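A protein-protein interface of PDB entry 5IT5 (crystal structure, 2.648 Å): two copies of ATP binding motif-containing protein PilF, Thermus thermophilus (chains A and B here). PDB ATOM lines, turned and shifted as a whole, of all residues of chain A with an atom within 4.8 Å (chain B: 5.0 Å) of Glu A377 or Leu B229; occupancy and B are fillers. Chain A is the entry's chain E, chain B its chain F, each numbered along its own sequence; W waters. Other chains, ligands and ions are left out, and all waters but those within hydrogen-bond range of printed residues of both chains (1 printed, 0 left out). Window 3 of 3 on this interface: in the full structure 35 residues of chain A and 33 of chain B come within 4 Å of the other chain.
Glu A377 touches Leu B229.
Leu A380 touches Leu B229.
CD2 of Leu A380 touches OD1 of Asn B259, 3.5 Å away.
Ala B262 touches Leu A380 (CB to CD1, 3.9 Å).
Glu B226 touches Ala A381.
CB of Ala A381 touches CB of Leu B229, at 3.7 Å.
OG1 of Thr B230 touches CB of Ala A381, at 3.7 Å.
Thr B225 touches Ile A384 (CB to CD1, 3.996 Å).
CB of Glu B226 touches CG2 of Ile A384 (3.7 Å).
Ile A384 touches Asn B259.
Water W1 lies within hydrogen-bond range of the backbone carbonyl oxygen (O) of Leu A380, the side-chain amide oxygen (OD1) of Asn B259 and the backbone NH (N) of Ile A384.
Of the 8 printed residues of chain A, 4 touch a printed residue of chain B.
Among the printed residues, no Asp or Glu carboxylate lies within 4 Å of a Lys or Arg side-chain nitrogen of the other chain.
The backbone carbonyl oxygen of Glu B226 lies within hydrogen-bond range of the side-chain hydroxyl of Thr B230.
Of the printed residues of chain A, Leu B229 touches Glu A377 (3.8 Å), Leu A380 (3.9 Å) and Ala A381 (3.7 Å).
Of the printed residues of chain A, Thr B230 touches Ala A381 (3.7 Å).
Of the printed residues of chain B, Ile A384 touches Thr B225, Glu B226 and Asn B259.
Leu A376 touches none of the printed residues of chain B.
Glu A378 touches none of the printed residues of chain B.
The nearest residue of chain B that does not touch Glu A377 is Ala B262 (4.5 Å).
No position is printed for both chains.
Of the 10 pairs that touch across the chains among the printed residues, none has its exchanged pair printed and touching as well.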
ATOM      1  N   THR A 375       5.430 -14.847 -25.260  1.00  0.00           N
ATOM      2  CA  THR A 375       4.846 -14.502 -23.975  1.00  0.00           C
ATOM      3  C   THR A 375       3.416 -14.062 -24.180  1.00  0.00           C
ATOM      4  O   THR A 375       3.009 -13.768 -25.301  1.00  0.00           O
ATOM      5  CB  THR A 375       5.624 -13.377 -23.276  1.00  0.00           C
ATOM      6  OG1 THR A 375       5.691 -12.228 -24.135  1.00  0.00           O
ATOM      7  CG2 THR A 375       7.029 -13.840 -22.948  1.00  0.00           C
ATOM      8  N   LEU A 376       2.651 -14.007 -23.099  1.00  0.00           N
ATOM      9  CA  LEU A 376       1.288 -13.496 -23.171  1.00  0.00           C
ATOM     10  C   LEU A 376       1.279 -11.974 -23.344  1.00  0.00           C
ATOM     11  O   LEU A 376       0.340 -11.415 -23.930  1.00  0.00           O
ATOM     12  CB  LEU A 376       0.501 -13.896 -21.926  1.00  0.00           C
ATOM     13  CG  LEU A 376      -0.988 -13.544 -21.966  1.00  0.00           C
ATOM     14  CD1 LEU A 376      -1.617 -14.207 -23.138  1.00  0.00           C
ATOM     15  CD2 LEU A 376      -1.671 -14.007 -20.706  1.00  0.00           C
ATOM     16  N   GLU A 377       2.330 -11.317 -22.848  1.00  0.00           N
ATOM     17  CA  GLU A 377       2.480  -9.860 -22.972  1.00  0.00           C
ATOM     18  C   GLU A 377       2.554  -9.424 -24.427  1.00  0.00           C
ATOM     19  O   GLU A 377       1.840  -8.506 -24.838  1.00  0.00           O
ATOM     20  CB  GLU A 377       3.733  -9.360 -22.236  1.00  0.00           C
ATOM     21  CG  GLU A 377       3.559  -9.133 -20.745  1.00  0.00           C
ATOM     22  CD  GLU A 377       3.495 -10.431 -19.962  1.00  0.00           C
ATOM     23  OE1 GLU A 377       3.789 -11.501 -20.553  1.00  0.00           O
ATOM     24  OE2 GLU A 377       3.143 -10.380 -18.759  1.00  0.00           O
ATOM     25  N   GLU A 378       3.432 -10.072 -25.192  1.00  0.00           N
ATOM     26  CA  GLU A 378       3.603  -9.763 -26.607  1.00  0.00           C
ATOM     27  C   GLU A 378       2.279  -9.998 -27.336  1.00  0.00           C
ATOM     28  O   GLU A 378       1.863  -9.210 -28.189  1.00  0.00           O
ATOM     29  CB  GLU A 378       4.739 -10.609 -27.201  1.00  0.00           C
ATOM     30  CG  GLU A 378       5.600  -9.898 -28.238  1.00  0.00           C
ATOM     31  CD  GLU A 378       6.357  -8.742 -27.659  1.00  0.00           C
ATOM     32  OE1 GLU A 378       6.540  -8.712 -26.414  1.00  0.00           O
ATOM     33  OE2 GLU A 378       6.748  -7.847 -28.441  1.00  0.00           O
ATOM     34  N   VAL A 379       1.587 -11.062 -26.962  1.00  0.00           N
ATOM     35  CA  VAL A 379       0.271 -11.296 -27.521  1.00  0.00           C
ATOM     36  C   VAL A 379      -0.698 -10.173 -27.174  1.00  0.00           C
ATOM     37  O   VAL A 379      -1.416  -9.702 -28.054  1.00  0.00           O
ATOM     38  CB  VAL A 379      -0.310 -12.639 -27.063  1.00  0.00           C
ATOM     39  CG1 VAL A 379      -1.765 -12.738 -27.436  1.00  0.00           C
ATOM     40  CG2 VAL A 379       0.443 -13.768 -27.720  1.00  0.00           C
ATOM     41  N   LEU A 380      -0.715  -9.718 -25.922  1.00  0.00           N
ATOM     42  CA  LEU A 380      -1.649  -8.650 -25.529  1.00  0.00           C
ATOM     43  C   LEU A 380      -1.308  -7.346 -26.213  1.00  0.00           C
ATOM     44  O   LEU A 380      -2.183  -6.601 -26.658  1.00  0.00           O
ATOM     45  CB  LEU A 380      -1.650  -8.444 -24.018  1.00  0.00           C
ATOM     46  CG  LEU A 380      -2.177  -9.605 -23.180  1.00  0.00           C
ATOM     47  CD1 LEU A 380      -2.074  -9.247 -21.719  1.00  0.00           C
ATOM     48  CD2 LEU A 380      -3.608  -9.984 -23.563  1.00  0.00           C
ATOM     49  N   ALA A 381      -0.018  -7.077 -26.281  1.00  0.00           N
ATOM     50  CA  ALA A 381       0.468  -5.853 -26.888  1.00  0.00           C
ATOM     51  C   ALA A 381      -0.013  -5.721 -28.320  1.00  0.00           C
ATOM     52  O   ALA A 381      -0.410  -4.640 -28.732  1.00  0.00           O
ATOM     53  CB  ALA A 381       1.988  -5.799 -26.829  1.00  0.00           C
ATOM     54  N   ILE A 384      -4.363  -5.417 -28.567  1.00  0.00           N
ATOM     55  CA  ILE A 384      -5.116  -4.405 -27.820  1.00  0.00           C
ATOM     56  C   ILE A 384      -5.685  -3.322 -28.758  1.00  0.00           C
ATOM     57  O   ILE A 384      -4.961  -2.521 -29.374  1.00  0.00           O
ATOM     58  CB  ILE A 384      -4.260  -3.760 -26.666  1.00  0.00           C
ATOM     59  CG1 ILE A 384      -5.072  -2.732 -25.889  1.00  0.00           C
ATOM     60  CG2 ILE A 384      -2.945  -3.139 -27.159  1.00  0.00           C
ATOM     61  CD1 ILE A 384      -4.390  -2.289 -24.594  1.00  0.00           C
ATOM     62  N   THR B 225      -1.008   1.870 -22.766  1.00  0.00           N
ATOM     63  CA  THR B 225      -1.003   0.524 -22.206  1.00  0.00           C
ATOM     64  C   THR B 225      -0.248  -0.424 -23.135  1.00  0.00           C
ATOM     65  O   THR B 225       0.477  -1.308 -22.685  1.00  0.00           O
ATOM     66  CB  THR B 225      -2.420   0.005 -21.982  1.00  0.00           C
ATOM     67  OG1 THR B 225      -3.148   0.960 -21.204  1.00  0.00           O
ATOM     68  CG2 THR B 225      -2.398  -1.308 -21.237  1.00  0.00           C
ATOM     69  N   GLU B 226      -0.410  -0.228 -24.437  1.00  0.00           N
ATOM     70  CA  GLU B 226       0.274  -1.060 -25.406  1.00  0.00           C
ATOM     71  C   GLU B 226       1.798  -0.874 -25.292  1.00  0.00           C
ATOM     72  O   GLU B 226       2.556  -1.841 -25.386  1.00  0.00           O
ATOM     73  CB  GLU B 226      -0.207  -0.740 -26.826  1.00  0.00           C
ATOM     74  CG  GLU B 226       0.500  -1.556 -27.906  1.00  0.00           C
ATOM     75  CD  GLU B 226       0.213  -1.067 -29.319  1.00  0.00           C
ATOM     76  OE1 GLU B 226      -0.539  -0.076 -29.481  1.00  0.00           O
ATOM     77  OE2 GLU B 226       0.740  -1.681 -30.278  1.00  0.00           O
ATOM     78  N   ALA B 227       2.255   0.359 -25.097  1.00  0.00           N
ATOM     79  CA  ALA B 227       3.687   0.590 -24.934  1.00  0.00           C
ATOM     80  C   ALA B 227       4.169  -0.161 -23.700  1.00  0.00           C
ATOM     81  O   ALA B 227       5.231  -0.780 -23.707  1.00  0.00           O
ATOM     82  CB  ALA B 227       4.001   2.082 -24.816  1.00  0.00           C
ATOM     83  N   ALA B 228       3.363  -0.125 -22.649  1.00  0.00           N
ATOM     84  CA  ALA B 228       3.724  -0.823 -21.431  1.00  0.00           C
ATOM     85  C   ALA B 228       3.834  -2.339 -21.660  1.00  0.00           C
ATOM     86  O   ALA B 228       4.761  -2.972 -21.148  1.00  0.00           O
ATOM     87  CB  ALA B 228       2.733  -0.514 -20.343  1.00  0.00           C
ATOM     88  N   LEU B 229       2.903  -2.905 -22.436  1.00  0.00           N
ATOM     89  CA  LEU B 229       2.906  -4.329 -22.764  1.00  0.00           C
ATOM     90  C   LEU B 229       4.044  -4.748 -23.733  1.00  0.00           C
ATOM     91  O   LEU B 229       4.469  -5.909 -23.749  1.00  0.00           O
ATOM     92  CB  LEU B 229       1.564  -4.704 -23.362  1.00  0.00           C
ATOM     93  CG  LEU B 229       0.400  -4.600 -22.384  1.00  0.00           C
ATOM     94  CD1 LEU B 229      -0.919  -4.738 -23.132  1.00  0.00           C
ATOM     95  CD2 LEU B 229       0.524  -5.650 -21.294  1.00  0.00           C
ATOM     96  N   THR B 230       4.526  -3.793 -24.527  1.00  0.00           N
ATOM     97  CA  THR B 230       5.560  -4.039 -25.517  1.00  0.00           C
ATOM     98  C   THR B 230       6.940  -4.129 -24.882  1.00  0.00           C
ATOM     99  O   THR B 230       7.868  -4.687 -25.471  1.00  0.00           O
ATOM    100  CB  THR B 230       5.549  -2.941 -26.612  1.00  0.00           C
ATOM    101  OG1 THR B 230       4.230  -2.831 -27.146  1.00  0.00           O
ATOM    102  CG2 THR B 230       6.514  -3.269 -27.774  1.00  0.00           C
ATOM    103  N   GLY B 231       7.077  -3.594 -23.672  1.00  0.00           N
ATOM    104  CA  GLY B 231       8.311  -3.730 -22.919  1.00  0.00           C
ATOM    105  C   GLY B 231       8.947  -2.418 -22.512  1.00  0.00           C
ATOM    106  O   GLY B 231      10.104  -2.388 -22.090  1.00  0.00           O
ATOM    107  N   ASN B 259      -5.414  -6.507 -19.519  1.00  0.00           N
ATOM    108  CA  ASN B 259      -4.314  -5.670 -19.985  1.00  0.00           C
ATOM    109  C   ASN B 259      -3.803  -4.774 -18.850  1.00  0.00           C
ATOM    110  O   ASN B 259      -2.598  -4.549 -18.722  1.00  0.00           O
ATOM    111  CB  ASN B 259      -4.730  -4.807 -21.181  1.00  0.00           C
ATOM    112  CG  ASN B 259      -5.065  -5.626 -22.415  1.00  0.00           C
ATOM    113  OD1 ASN B 259      -4.447  -6.650 -22.692  1.00  0.00           O
ATOM    114  ND2 ASN B 259      -6.058  -5.170 -23.160  1.00  0.00           N
ATOM    115  N   ALA B 262      -1.594  -6.765 -16.483  1.00  0.00           N
ATOM    116  CA  ALA B 262      -0.312  -7.128 -17.075  1.00  0.00           C
ATOM    117  C   ALA B 262       0.671  -5.952 -17.261  1.00  0.00           C
ATOM    118  O   ALA B 262       1.873  -6.178 -17.397  1.00  0.00           O
ATOM    119  CB  ALA B 262      -0.549  -7.821 -18.418  1.00  0.00           C
ATOM    120  N   ALA B 263       0.173  -4.719 -17.267  1.00  0.00           N
ATOM    121  CA  ALA B 263       0.997  -3.552 -17.565  1.00  0.00           C
ATOM    122  C   ALA B 263       1.205  -2.592 -16.380  1.00  0.00           C
ATOM    123  O   ALA B 263       2.203  -1.876 -16.336  1.00  0.00           O
ATOM    124  CB  ALA B 263       0.398  -2.799 -18.711  1.00  0.00           C
HETATM  125  O   HOH W   1      -4.800  -6.968 -25.722  1.00  0.00           O
